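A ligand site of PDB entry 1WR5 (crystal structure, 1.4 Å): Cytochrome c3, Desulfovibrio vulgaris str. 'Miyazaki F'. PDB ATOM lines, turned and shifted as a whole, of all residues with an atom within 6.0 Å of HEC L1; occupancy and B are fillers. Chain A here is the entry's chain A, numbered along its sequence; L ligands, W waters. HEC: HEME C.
Water W4 bridges O2A of HEC L1 (2.4 Å) and O of Met 56 (2.9 Å). Water W2 bridges O2A of HEC L1 (2.6 Å) and SD of Met 56 (3.6 Å). Water W1 bridges an oxygen (O1A) of HEC L1 and the backbone NH (N) of Lys 16.
N of Met 12 sits at hydrogen-bond distance from O of Val 19, at 2.7 Å. A ring nitrogen (ND1) of His 84 is in hydrogen-bond range of the backbone carbonyl oxygen (O) of Leu 98 (2.8 Å). The backbone NH (N) of His 107 lies within hydrogen-bond range of the side-chain hydroxyl (OG) of Ser 104. A ring nitrogen (ND1) of His 71 is in hydrogen-bond range of the backbone carbonyl oxygen (O) of Tyr 67. The backbone carbonyl oxygen (O) of Gly 100 sits at hydrogen-bond distance from the side-chain hydroxyl (OG) of Ser 104, 2.6 Å away. The backbone NH (N) of Cys 106 lies close to the side-chain hydroxyl (OG) of Ser 104. The side-chain hydroxyl of Thr 15 sits close to the backbone NH of Gln 17, 3.4 Å away. N of Cys 80 lies close to O of Met 70.
The side-chain sulfur (SG) of Cys 106 is bonded to a carbon (CAC) of HEC L1, 1.8 Å away. FE of HEC L2 is bound by NE2 of His 84, 1.9 Å away. CAB of HEC L1 is bonded to SG of Cys 101. The backbone NH of Asp 13 is in hydrogen-bond range of an oxygen (O1D) of HEC L1 (3.3 Å). SG of Cys 80 is covalently linked to CAB of HEC L2 (1.8 Å). The side-chain hydroxyl of Thr 15 sits at hydrogen-bond distance from an oxygen (O2D) of HEC L1 (2.6 Å). The side-chain hydroxyl of Tyr 66 is in hydrogen-bond range of an oxygen (O1D) of HEC L1, 2.6 Å away. O1D of HEC L1 lies within hydrogen-bond range of N of Lys 14, 2.9 Å away. The backbone NH (N) of Thr 15 is in hydrogen-bond range of an oxygen (O2D) of HEC L1. An iron atom (FE) of HEC L1 is bound by a ring nitrogen (NE2) of His 71 (1.9 Å). NE2 of His 107 binds FE of HEC L1, at 1.9 Å.
The backbone carbonyl oxygen of Met 12 sits close to an oxygen (O2D) of HEC L1, 3.2 Å away. Merely in contact with HEC L1: Leu 98 (3.3 Å), His 84 (3.4 Å), Thr 99 (3.4 Å), Tyr 67 (3.5 Å), Gly 100 (3.5 Å), Pro 18 (3.5 Å), Val 19 (3.5 Å), Gln 17 (3.6 Å), Cys 80 (3.6 Å), Lys 58 (3.6 Å), Val 81 (3.6 Å), Met 70 (3.8 Å) and Met 56 (3.98 Å).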
ATOM      1  N   MET A  12       8.067  13.099 -32.722  1.00  0.00           N
ATOM      2  CA  MET A  12       8.742  13.945 -31.766  1.00  0.00           C
ATOM      3  C   MET A  12      10.214  13.541 -31.833  1.00  0.00           C
ATOM      4  O   MET A  12      10.523  12.418 -31.425  1.00  0.00           O
ATOM      5  CB  MET A  12       8.148  13.786 -30.359  1.00  0.00           C
ATOM      6  CG  MET A  12       6.648  14.042 -30.344  1.00  0.00           C
ATOM      7  SD  MET A  12       5.898  13.747 -28.725  1.00  0.00           S
ATOM      8  CE  MET A  12       6.419  15.217 -27.867  1.00  0.00           C
ATOM      9  N   ASP A  13      11.059  14.412 -32.370  1.00  0.00           N
ATOM     10  CA  ASP A  13      12.443  13.995 -32.638  1.00  0.00           C
ATOM     11  C   ASP A  13      13.452  15.063 -32.278  1.00  0.00           C
ATOM     12  O   ASP A  13      14.394  15.325 -33.027  1.00  0.00           O
ATOM     13  CB  ASP A  13      12.611  13.594 -34.099  1.00  0.00           C
ATOM     14  CG  ASP A  13      12.295  14.691 -35.071  1.00  0.00           C
ATOM     15  OD1 ASP A  13      11.933  15.792 -34.606  1.00  0.00           O
ATOM     16  OD2 ASP A  13      12.441  14.402 -36.268  1.00  0.00           O
ATOM     17  N   LYS A  14      13.225  15.674 -31.107  1.00  0.00           N
ATOM     18  CA  LYS A  14      14.195  16.594 -30.543  1.00  0.00           C
ATOM     19  C   LYS A  14      15.419  15.840 -30.025  1.00  0.00           C
ATOM     20  O   LYS A  14      16.521  16.378 -29.866  1.00  0.00           O
ATOM     21  CB  LYS A  14      13.499  17.443 -29.472  1.00  0.00           C
ATOM     22  CG  LYS A  14      12.840  18.630 -30.232  1.00  0.00           C
ATOM     23  CD  LYS A  14      13.814  19.792 -30.397  1.00  0.00           C
ATOM     24  CE  LYS A  14      13.401  20.886 -31.334  1.00  0.00           C
ATOM     25  NZ  LYS A  14      13.769  20.655 -32.767  1.00  0.00           N
ATOM     26  N   THR A  15      15.270  14.546 -29.735  1.00  0.00           N
ATOM     27  CA  THR A  15      16.307  13.718 -29.159  1.00  0.00           C
ATOM     28  C   THR A  15      16.684  12.511 -30.041  1.00  0.00           C
ATOM     29  O   THR A  15      16.107  12.314 -31.116  1.00  0.00           O
ATOM     30  CB  THR A  15      15.895  13.153 -27.766  1.00  0.00           C
ATOM     31  OG1 THR A  15      14.926  12.120 -28.009  1.00  0.00           O
ATOM     32  CG2 THR A  15      15.207  14.152 -26.871  1.00  0.00           C
ATOM     33  N   LYS A  16      17.623  11.714 -29.540  1.00  0.00           N
ATOM     34  CA  LYS A  16      18.164  10.539 -30.211  1.00  0.00           C
ATOM     35  C   LYS A  16      17.286   9.308 -30.081  1.00  0.00           C
ATOM     36  O   LYS A  16      17.371   8.247 -30.713  1.00  0.00           O
ATOM     37  CB  LYS A  16      19.550  10.182 -29.661  1.00  0.00           C
ATOM     38  CG  LYS A  16      20.729  10.945 -30.236  1.00  0.00           C
ATOM     39  CD  LYS A  16      20.293  12.300 -30.756  1.00  0.00           C
ATOM     40  CE  LYS A  16      20.456  12.461 -32.263  1.00  0.00           C
ATOM     41  NZ  LYS A  16      21.403  13.555 -32.598  1.00  0.00           N
ATOM     42  N   GLN A  17      16.356   9.323 -29.173  1.00  0.00           N
ATOM     43  CA  GLN A  17      15.198   8.476 -28.966  1.00  0.00           C
ATOM     44  C   GLN A  17      13.856   9.057 -29.390  1.00  0.00           C
ATOM     45  O   GLN A  17      13.003   9.300 -28.521  1.00  0.00           O
ATOM     46  CB  GLN A  17      15.169   8.159 -27.451  1.00  0.00           C
ATOM     47  CG  GLN A  17      16.505   7.639 -26.970  1.00  0.00           C
ATOM     48  CD  GLN A  17      16.874   6.259 -27.437  1.00  0.00           C
ATOM     49  OE1 GLN A  17      17.994   5.814 -27.103  1.00  0.00           O
ATOM     50  NE2 GLN A  17      16.017   5.541 -28.141  1.00  0.00           N
ATOM     51  N   PRO A  18      13.607   9.299 -30.663  1.00  0.00           N
ATOM     52  CA  PRO A  18      12.343   9.902 -31.071  1.00  0.00           C
ATOM     53  C   PRO A  18      11.124   9.003 -30.856  1.00  0.00           C
ATOM     54  O   PRO A  18      11.172   7.780 -30.812  1.00  0.00           O
ATOM     55  CB  PRO A  18      12.541  10.171 -32.569  1.00  0.00           C
ATOM     56  CG  PRO A  18      13.559   9.174 -32.970  1.00  0.00           C
ATOM     57  CD  PRO A  18      14.497   9.042 -31.798  1.00  0.00           C
ATOM     58  N   VAL A  19       9.980   9.635 -30.702  1.00  0.00           N
ATOM     59  CA  VAL A  19       8.723   8.998 -30.356  1.00  0.00           C
ATOM     60  C   VAL A  19       7.607   9.489 -31.257  1.00  0.00           C
ATOM     61  O   VAL A  19       7.499  10.691 -31.556  1.00  0.00           O
ATOM     62  CB  VAL A  19       8.410   9.304 -28.859  1.00  0.00           C
ATOM     63  CG1 VAL A  19       7.065   8.725 -28.461  1.00  0.00           C
ATOM     64  CG2 VAL A  19       9.516   8.792 -27.950  1.00  0.00           C
ATOM     65  N   MET A  56      17.414  20.589 -23.129  1.00  0.00           N
ATOM     66  CA  MET A  56      17.715  19.235 -23.560  1.00  0.00           C
ATOM     67  C   MET A  56      18.584  18.468 -22.562  1.00  0.00           C
ATOM     68  O   MET A  56      19.038  17.375 -22.908  1.00  0.00           O
ATOM     69  CB  MET A  56      18.312  19.284 -24.968  1.00  0.00           C
ATOM     70  CG  MET A  56      17.329  19.827 -26.005  1.00  0.00           C
ATOM     71  SD  MET A  56      15.936  18.684 -26.225  1.00  0.00           S
ATOM     72  CE  MET A  56      14.625  19.866 -26.008  1.00  0.00           C
ATOM     73  N   ASP A  57      18.771  19.010 -21.370  1.00  0.00           N
ATOM     74  CA  ASP A  57      19.407  18.333 -20.257  1.00  0.00           C
ATOM     75  C   ASP A  57      18.380  17.417 -19.617  1.00  0.00           C
ATOM     76  O   ASP A  57      17.473  17.918 -18.950  1.00  0.00           O
ATOM     77  CB  ASP A  57      19.949  19.351 -19.266  1.00  0.00           C
ATOM     78  CG  ASP A  57      20.593  18.767 -18.032  1.00  0.00           C
ATOM     79  OD1 ASP A  57      20.703  17.533 -17.948  1.00  0.00           O
ATOM     80  OD2 ASP A  57      20.971  19.573 -17.142  1.00  0.00           O
ATOM     81  N   LYS A  58      18.515  16.111 -19.829  1.00  0.00           N
ATOM     82  CA  LYS A  58      17.473  15.170 -19.371  1.00  0.00           C
ATOM     83  C   LYS A  58      17.483  15.047 -17.845  1.00  0.00           C
ATOM     84  O   LYS A  58      16.553  14.439 -17.275  1.00  0.00           O
ATOM     85  CB  LYS A  58      17.614  13.798 -20.010  1.00  0.00           C
ATOM     86  CG  LYS A  58      18.760  12.876 -19.709  1.00  0.00           C
ATOM     87  CD  LYS A  58      18.670  11.583 -20.505  1.00  0.00           C
ATOM     88  CE  LYS A  58      20.009  10.846 -20.406  1.00  0.00           C
ATOM     89  NZ  LYS A  58      19.890   9.458 -20.902  1.00  0.00           N
ATOM     90  N   TYR A  66      12.776  19.231 -21.082  1.00  0.00           N
ATOM     91  CA  TYR A  66      12.013  18.448 -22.032  1.00  0.00           C
ATOM     92  C   TYR A  66      11.805  17.026 -21.540  1.00  0.00           C
ATOM     93  O   TYR A  66      10.659  16.519 -21.570  1.00  0.00           O
ATOM     94  CB  TYR A  66      12.717  18.452 -23.389  1.00  0.00           C
ATOM     95  CG  TYR A  66      11.952  17.787 -24.525  1.00  0.00           C
ATOM     96  CD1 TYR A  66      12.543  16.777 -25.268  1.00  0.00           C
ATOM     97  CD2 TYR A  66      10.679  18.170 -24.898  1.00  0.00           C
ATOM     98  CE1 TYR A  66      11.895  16.163 -26.319  1.00  0.00           C
ATOM     99  CE2 TYR A  66       9.997  17.584 -25.935  1.00  0.00           C
ATOM    100  CZ  TYR A  66      10.627  16.568 -26.642  1.00  0.00           C
ATOM    101  OH  TYR A  66       9.946  15.994 -27.661  1.00  0.00           O
ATOM    102  N   TYR A  67      12.892  16.382 -21.134  1.00  0.00           N
ATOM    103  CA  TYR A  67      12.740  14.985 -20.653  1.00  0.00           C
ATOM    104  C   TYR A  67      11.721  14.965 -19.523  1.00  0.00           C
ATOM    105  O   TYR A  67      10.826  14.109 -19.443  1.00  0.00           O
ATOM    106  CB  TYR A  67      14.096  14.463 -20.197  1.00  0.00           C
ATOM    107  CG  TYR A  67      14.030  13.048 -19.672  1.00  0.00           C
ATOM    108  CD1 TYR A  67      13.768  12.721 -18.356  1.00  0.00           C
ATOM    109  CD2 TYR A  67      14.265  11.972 -20.524  1.00  0.00           C
ATOM    110  CE1 TYR A  67      13.709  11.438 -17.907  1.00  0.00           C
ATOM    111  CE2 TYR A  67      14.218  10.676 -20.115  1.00  0.00           C
ATOM    112  CZ  TYR A  67      13.926  10.422 -18.793  1.00  0.00           C
ATOM    113  OH  TYR A  67      13.888   9.106 -18.361  1.00  0.00           O
ATOM    114  N   MET A  70       8.105  15.121 -20.382  1.00  0.00           N
ATOM    115  CA  MET A  70       7.571  13.936 -21.042  1.00  0.00           C
ATOM    116  C   MET A  70       7.491  12.705 -20.145  1.00  0.00           C
ATOM    117  O   MET A  70       6.711  11.772 -20.426  1.00  0.00           O
ATOM    118  CB  MET A  70       8.349  13.585 -22.330  1.00  0.00           C
ATOM    119  CG  MET A  70       8.458  14.746 -23.303  1.00  0.00           C
ATOM    120  SD  MET A  70       6.866  15.324 -23.894  1.00  0.00           S
ATOM    121  CE  MET A  70       6.886  17.036 -23.415  1.00  0.00           C
ATOM    122  N   HIS A  71       8.267  12.637 -19.076  1.00  0.00           N
ATOM    123  CA  HIS A  71       8.410  11.398 -18.296  1.00  0.00           C
ATOM    124  C   HIS A  71       8.019  11.460 -16.804  1.00  0.00           C
ATOM    125  O   HIS A  71       7.813  10.407 -16.230  1.00  0.00           O
ATOM    126  CB  HIS A  71       9.883  10.905 -18.352  1.00  0.00           C
ATOM    127  CG  HIS A  71      10.356  10.575 -19.720  1.00  0.00           C
ATOM    128  ND1 HIS A  71      10.834  11.533 -20.627  1.00  0.00           N
ATOM    129  CD2 HIS A  71      10.448   9.424 -20.399  1.00  0.00           C
ATOM    130  CE1 HIS A  71      11.155  10.923 -21.745  1.00  0.00           C
ATOM    131  NE2 HIS A  71      10.941   9.597 -21.671  1.00  0.00           N
ATOM    132  N   CYS A  80       3.483  12.427 -20.476  1.00  0.00           N
ATOM    133  CA  CYS A  80       3.198  11.224 -21.220  1.00  0.00           C
ATOM    134  C   CYS A  80       3.262  10.002 -20.306  1.00  0.00           C
ATOM    135  O   CYS A  80       2.293   9.252 -20.232  1.00  0.00           O
ATOM    136  CB  CYS A  80       4.207  11.011 -22.334  1.00  0.00           C
ATOM    137  SG  CYS A  80       4.670  12.369 -23.437  1.00  0.00           S
ATOM    138  N   VAL A  81       4.409   9.852 -19.626  1.00  0.00           N
ATOM    139  CA  VAL A  81       4.574   8.652 -18.792  1.00  0.00           C
ATOM    140  C   VAL A  81       3.687   8.721 -17.559  1.00  0.00           C
ATOM    141  O   VAL A  81       3.119   7.688 -17.182  1.00  0.00           O
ATOM    142  CB  VAL A  81       6.030   8.442 -18.381  1.00  0.00           C
ATOM    143  CG1 VAL A  81       6.190   7.236 -17.483  1.00  0.00           C
ATOM    144  CG2 VAL A  81       6.840   8.301 -19.652  1.00  0.00           C
ATOM    145  N   HIS A  84       0.219   7.730 -18.520  1.00  0.00           N
ATOM    146  CA  HIS A  84       0.234   6.311 -18.893  1.00  0.00           C
ATOM    147  C   HIS A  84       0.372   5.423 -17.691  1.00  0.00           C
ATOM    148  O   HIS A  84      -0.219   4.332 -17.689  1.00  0.00           O
ATOM    149  CB  HIS A  84       1.338   6.034 -19.905  1.00  0.00           C
ATOM    150  CG  HIS A  84       1.013   6.545 -21.266  1.00  0.00           C
ATOM    151  ND1 HIS A  84       1.756   6.098 -22.361  1.00  0.00           N
ATOM    152  CD2 HIS A  84       0.127   7.391 -21.795  1.00  0.00           C
ATOM    153  CE1 HIS A  84       1.309   6.673 -23.416  1.00  0.00           C
ATOM    154  NE2 HIS A  84       0.282   7.500 -23.160  1.00  0.00           N
ATOM    155  N   GLU A  97       3.512  -1.802 -22.557  1.00  0.00           N
ATOM    156  CA  GLU A  97       3.165  -1.095 -23.800  1.00  0.00           C
ATOM    157  C   GLU A  97       3.222   0.413 -23.637  1.00  0.00           C
ATOM    158  O   GLU A  97       3.666   1.168 -24.495  1.00  0.00           O
ATOM    159  CB  GLU A  97       1.782  -1.540 -24.248  1.00  0.00           C
ATOM    160  CG  GLU A  97       1.273  -1.000 -25.559  1.00  0.00           C
ATOM    161  CD  GLU A  97      -0.188  -1.262 -25.860  1.00  0.00           C
ATOM    162  OE1 GLU A  97      -0.698  -0.737 -26.866  1.00  0.00           O
ATOM    163  OE2 GLU A  97      -0.869  -1.954 -25.072  1.00  0.00           O
ATOM    164  N   LEU A  98       2.747   0.879 -22.483  1.00  0.00           N
ATOM    165  CA  LEU A  98       2.511   2.309 -22.317  1.00  0.00           C
ATOM    166  C   LEU A  98       3.587   3.022 -21.506  1.00  0.00           C
ATOM    167  O   LEU A  98       3.677   4.251 -21.570  1.00  0.00           O
ATOM    168  CB  LEU A  98       1.155   2.578 -21.660  1.00  0.00           C
ATOM    169  CG  LEU A  98      -0.078   2.018 -22.406  1.00  0.00           C
ATOM    170  CD1 LEU A  98      -1.337   2.355 -21.595  1.00  0.00           C
ATOM    171  CD2 LEU A  98      -0.144   2.564 -23.826  1.00  0.00           C
ATOM    172  N   THR A  99       4.357   2.301 -20.707  1.00  0.00           N
ATOM    173  CA  THR A  99       5.315   2.981 -19.828  1.00  0.00           C
ATOM    174  C   THR A  99       6.711   2.393 -19.918  1.00  0.00           C
ATOM    175  O   THR A  99       7.615   2.913 -19.303  1.00  0.00           O
ATOM    176  CB  THR A  99       4.929   2.967 -18.323  1.00  0.00           C
ATOM    177  OG1 THR A  99       5.078   1.683 -17.722  1.00  0.00           O
ATOM    178  CG2 THR A  99       3.497   3.406 -18.139  1.00  0.00           C
ATOM    179  N   GLY A 100       6.905   1.325 -20.695  1.00  0.00           N
ATOM    180  CA  GLY A 100       8.196   0.726 -20.742  1.00  0.00           C
ATOM    181  C   GLY A 100       9.254   1.625 -21.359  1.00  0.00           C
ATOM    182  O   GLY A 100       8.977   2.392 -22.272  1.00  0.00           O
ATOM    183  N   CYS A 101      10.478   1.505 -20.833  1.00  0.00           N
ATOM    184  CA  CYS A 101      11.563   2.327 -21.298  1.00  0.00           C
ATOM    185  C   CYS A 101      12.162   1.830 -22.601  1.00  0.00           C
ATOM    186  O   CYS A 101      12.783   2.622 -23.317  1.00  0.00           O
ATOM    187  CB  CYS A 101      12.635   2.403 -20.225  1.00  0.00           C
ATOM    188  SG  CYS A 101      12.114   3.016 -18.638  1.00  0.00           S
ATOM    189  N   LYS A 102      11.927   0.546 -22.840  1.00  0.00           N
ATOM    190  CA  LYS A 102      12.228  -0.036 -24.149  1.00  0.00           C
ATOM    191  C   LYS A 102      11.167  -1.091 -24.458  1.00  0.00           C
ATOM    192  O   LYS A 102      10.460  -1.495 -23.522  1.00  0.00           O
ATOM    193  CB  LYS A 102      13.625  -0.646 -24.182  1.00  0.00           C
ATOM    194  CG  LYS A 102      13.861  -1.705 -23.134  1.00  0.00           C
ATOM    195  CD  LYS A 102      15.338  -2.116 -23.213  1.00  0.00           C
ATOM    196  CE  LYS A 102      15.634  -3.103 -22.089  1.00  0.00           C
ATOM    197  NZ  LYS A 102      16.603  -4.121 -22.584  1.00  0.00           N
ATOM    198  N   SER A 104       8.427  -0.672 -25.830  1.00  0.00           N
ATOM    199  CA  SER A 104       7.102  -0.078 -25.619  1.00  0.00           C
ATOM    200  C   SER A 104       6.614   0.634 -26.878  1.00  0.00           C
ATOM    201  O   SER A 104       7.302   0.745 -27.887  1.00  0.00           O
ATOM    202  CB  SER A 104       7.084   0.894 -24.444  1.00  0.00           C
ATOM    203  OG  SER A 104       7.838   2.054 -24.599  1.00  0.00           O
ATOM    204  N   LYS A 105       5.373   1.141 -26.835  1.00  0.00           N
ATOM    205  CA  LYS A 105       4.903   1.861 -28.013  1.00  0.00           C
ATOM    206  C   LYS A 105       5.496   3.237 -28.134  1.00  0.00           C
ATOM    207  O   LYS A 105       5.444   3.870 -29.209  1.00  0.00           O
ATOM    208  CB  LYS A 105       3.370   1.957 -27.940  1.00  0.00           C
ATOM    209  CG  LYS A 105       2.795   0.569 -28.240  1.00  0.00           C
ATOM    210  CD  LYS A 105       1.838   0.551 -29.398  1.00  0.00           C
ATOM    211  CE  LYS A 105       1.098  -0.782 -29.526  1.00  0.00           C
ATOM    212  NZ  LYS A 105      -0.372  -0.615 -29.323  1.00  0.00           N
ATOM    213  N   CYS A 106       6.110   3.755 -27.073  1.00  0.00           N
ATOM    214  CA  CYS A 106       6.921   4.951 -27.261  1.00  0.00           C
ATOM    215  C   CYS A 106       8.329   4.703 -27.771  1.00  0.00           C
ATOM    216  O   CYS A 106       8.808   5.299 -28.712  1.00  0.00           O
ATOM    217  CB  CYS A 106       7.031   5.706 -25.931  1.00  0.00           C
ATOM    218  SG  CYS A 106       5.429   6.264 -25.329  1.00  0.00           S
ATOM    219  N   HIS A 107       9.144   3.863 -27.161  1.00  0.00           N
ATOM    220  CA  HIS A 107      10.490   3.468 -27.423  1.00  0.00           C
ATOM    221  C   HIS A 107      10.567   1.986 -27.759  1.00  0.00           C
ATOM    222  O   HIS A 107      10.472   1.122 -26.907  1.00  0.00           O
ATOM    223  CB  HIS A 107      11.404   3.741 -26.236  1.00  0.00           C
ATOM    224  CG  HIS A 107      11.457   5.127 -25.711  1.00  0.00           C
ATOM    225  ND1 HIS A 107      11.836   6.232 -26.501  1.00  0.00           N
ATOM    226  CD2 HIS A 107      11.210   5.680 -24.512  1.00  0.00           C
ATOM    227  CE1 HIS A 107      11.789   7.293 -25.767  1.00  0.00           C
ATOM    228  NE2 HIS A 107      11.394   7.047 -24.500  1.00  0.00           N
HETATM  229 FE   HEC L   1      11.238   8.352 -23.102  1.00  0.00          FE
HETATM  230  CHA HEC L   1      12.914  10.714 -25.026  1.00  0.00           C
HETATM  231  CHB HEC L   1      14.188   7.352 -21.741  1.00  0.00           C
HETATM  232  CHC HEC L   1       9.698   5.851 -21.381  1.00  0.00           C
HETATM  233  CHD HEC L   1       8.348   9.421 -24.316  1.00  0.00           C
HETATM  234  NA  HEC L   1      13.235   8.964 -23.326  1.00  0.00           N
HETATM  235  C1A HEC L   1      13.676   9.881 -24.249  1.00  0.00           C
HETATM  236  C2A HEC L   1      15.094   9.840 -24.139  1.00  0.00           C
HETATM  237  C3A HEC L   1      15.470   8.978 -23.173  1.00  0.00           C
HETATM  238  C4A HEC L   1      14.275   8.361 -22.684  1.00  0.00           C
HETATM  239  CMA HEC L   1      16.829   8.664 -22.624  1.00  0.00           C
HETATM  240  CAA HEC L   1      15.999  10.844 -24.854  1.00  0.00           C
HETATM  241  CBA HEC L   1      16.487  11.954 -23.914  1.00  0.00           C
HETATM  242  CGA HEC L   1      17.638  12.824 -24.468  1.00  0.00           C
HETATM  243  O1A HEC L   1      18.484  12.303 -25.207  1.00  0.00           O
HETATM  244  O2A HEC L   1      17.479  14.059 -24.468  1.00  0.00           O
HETATM  245  NB  HEC L   1      11.842   6.893 -21.755  1.00  0.00           N
HETATM  246  C1B HEC L   1      13.056   6.888 -21.128  1.00  0.00           C
HETATM  247  C2B HEC L   1      13.078   5.868 -20.118  1.00  0.00           C
HETATM  248  C3B HEC L   1      11.807   5.381 -20.017  1.00  0.00           C
HETATM  249  C4B HEC L   1      11.023   6.084 -21.003  1.00  0.00           C
HETATM  250  CMB HEC L   1      14.307   5.611 -19.254  1.00  0.00           C
HETATM  251  CAB HEC L   1      11.233   4.593 -18.997  1.00  0.00           C
HETATM  252  CBB HEC L   1      10.843   5.153 -17.702  1.00  0.00           C
HETATM  253  NC  HEC L   1       9.250   7.730 -22.878  1.00  0.00           N
HETATM  254  C1C HEC L   1       8.905   6.567 -22.274  1.00  0.00           C
HETATM  255  C2C HEC L   1       7.526   6.313 -22.617  1.00  0.00           C
HETATM  256  C3C HEC L   1       7.097   7.374 -23.436  1.00  0.00           C
HETATM  257  C4C HEC L   1       8.210   8.241 -23.603  1.00  0.00           C
HETATM  258  CMC HEC L   1       6.789   5.078 -22.124  1.00  0.00           C
HETATM  259  CAC HEC L   1       5.809   7.485 -24.070  1.00  0.00           C
HETATM  260  CBC HEC L   1       4.727   7.561 -23.128  1.00  0.00           C
HETATM  261  ND  HEC L   1      10.715   9.843 -24.454  1.00  0.00           N
HETATM  262  C1D HEC L   1       9.410  10.180 -24.690  1.00  0.00           C
HETATM  263  C2D HEC L   1       9.384  11.364 -25.487  1.00  0.00           C
HETATM  264  C3D HEC L   1      10.675  11.697 -25.680  1.00  0.00           C
HETATM  265  C4D HEC L   1      11.522  10.726 -25.074  1.00  0.00           C
HETATM  266  CMD HEC L   1       8.124  12.064 -25.970  1.00  0.00           C
HETATM  267  CAD HEC L   1      11.173  12.767 -26.586  1.00  0.00           C
HETATM  268  CBD HEC L   1      11.192  12.352 -28.071  1.00  0.00           C
HETATM  269  CGD HEC L   1      11.920  13.319 -28.929  1.00  0.00           C
HETATM  270  O1D HEC L   1      11.494  14.486 -29.061  1.00  0.00           O
HETATM  271  O2D HEC L   1      12.993  12.947 -29.459  1.00  0.00           O
HETATM  272 FE   HEC L   2      -0.629   8.514 -24.541  1.00  0.00          FE
HETATM  273  CHA HEC L   2      -1.917   5.600 -25.776  1.00  0.00           C
HETATM  274  CHB HEC L   2       2.151   8.190 -26.533  1.00  0.00           C
HETATM  275  CHC HEC L   2       0.497  11.457 -23.536  1.00  0.00           C
HETATM  276  CHD HEC L   2      -3.311   8.815 -22.479  1.00  0.00           C
HETATM  277  NA  HEC L   2      -0.034   7.128 -25.979  1.00  0.00           N
HETATM  278  C1A HEC L   2      -0.637   5.934 -26.200  1.00  0.00           C
HETATM  279  C2A HEC L   2       0.204   5.211 -27.132  1.00  0.00           C
HETATM  280  C3A HEC L   2       1.359   5.925 -27.321  1.00  0.00           C
HETATM  281  C4A HEC L   2       1.188   7.207 -26.664  1.00  0.00           C
HETATM  282  CMA HEC L   2       2.565   5.590 -28.171  1.00  0.00           C
HETATM  283  CAA HEC L   2      -0.184   3.907 -27.750  1.00  0.00           C
HETATM  284  CBA HEC L   2      -1.206   4.066 -28.919  1.00  0.00           C
HETATM  285  CGA HEC L   2      -0.531   4.668 -30.152  1.00  0.00           C
HETATM  286  O1A HEC L   2       0.166   3.888 -30.827  1.00  0.00           O
HETATM  287  O2A HEC L   2      -0.749   5.898 -30.363  1.00  0.00           O
HETATM  288  NB  HEC L   2       1.115   9.617 -24.952  1.00  0.00           N
HETATM  289  C1B HEC L   2       2.124   9.355 -25.793  1.00  0.00           C
HETATM  290  C2B HEC L   2       3.087  10.408 -25.756  1.00  0.00           C
HETATM  291  C3B HEC L   2       2.628  11.344 -24.899  1.00  0.00           C
HETATM  292  C4B HEC L   2       1.325  10.892 -24.482  1.00  0.00           C
HETATM  293  CMB HEC L   2       4.400  10.333 -26.548  1.00  0.00           C
HETATM  294  CAB HEC L   2       3.238  12.613 -24.530  1.00  0.00           C
HETATM  295  CBB HEC L   2       3.589  13.611 -25.529  1.00  0.00           C
HETATM  296  NC  HEC L   2      -1.257   9.890 -23.075  1.00  0.00           N
HETATM  297  C1C HEC L   2      -0.603  11.047 -22.830  1.00  0.00           C
HETATM  298  C2C HEC L   2      -1.319  11.740 -21.769  1.00  0.00           C
HETATM  299  C3C HEC L   2      -2.415  10.943 -21.428  1.00  0.00           C
HETATM  300  C4C HEC L   2      -2.359   9.802 -22.303  1.00  0.00           C
HETATM  301  CMC HEC L   2      -0.776  13.049 -21.180  1.00  0.00           C
HETATM  302  CAC HEC L   2      -3.344  11.061 -20.348  1.00  0.00           C
HETATM  303  CBC HEC L   2      -3.710  12.362 -19.892  1.00  0.00           C
HETATM  304  ND  HEC L   2      -2.349   7.369 -24.182  1.00  0.00           N
HETATM  305  C1D HEC L   2      -3.278   7.652 -23.253  1.00  0.00           C
HETATM  306  C2D HEC L   2      -4.359   6.720 -23.392  1.00  0.00           C
HETATM  307  C3D HEC L   2      -3.978   5.856 -24.341  1.00  0.00           C
HETATM  308  C4D HEC L   2      -2.671   6.242 -24.821  1.00  0.00           C
HETATM  309  CMD HEC L   2      -5.604   6.723 -22.504  1.00  0.00           C
HETATM  310  CAD HEC L   2      -4.575   4.576 -24.821  1.00  0.00           C
HETATM  311  CBD HEC L   2      -4.107   3.377 -23.963  1.00  0.00           C
HETATM  312  CGD HEC L   2      -4.312   2.034 -24.608  1.00  0.00           C
HETATM  313  O1D HEC L   2      -4.266   1.011 -23.918  1.00  0.00           O
HETATM  314  O2D HEC L   2      -4.052   1.890 -25.831  1.00  0.00           O
HETATM  315  O   HOH W   1      19.322  13.117 -27.595  1.00  0.00           O
HETATM  316  O   HOH W   2      15.724  15.950 -23.956  1.00  0.00           O
HETATM  317  O   HOH W   3       9.531   7.958 -16.297  1.00  0.00           O
HETATM  318  O   HOH W   4      18.874  15.868 -25.339  1.00  0.00           O
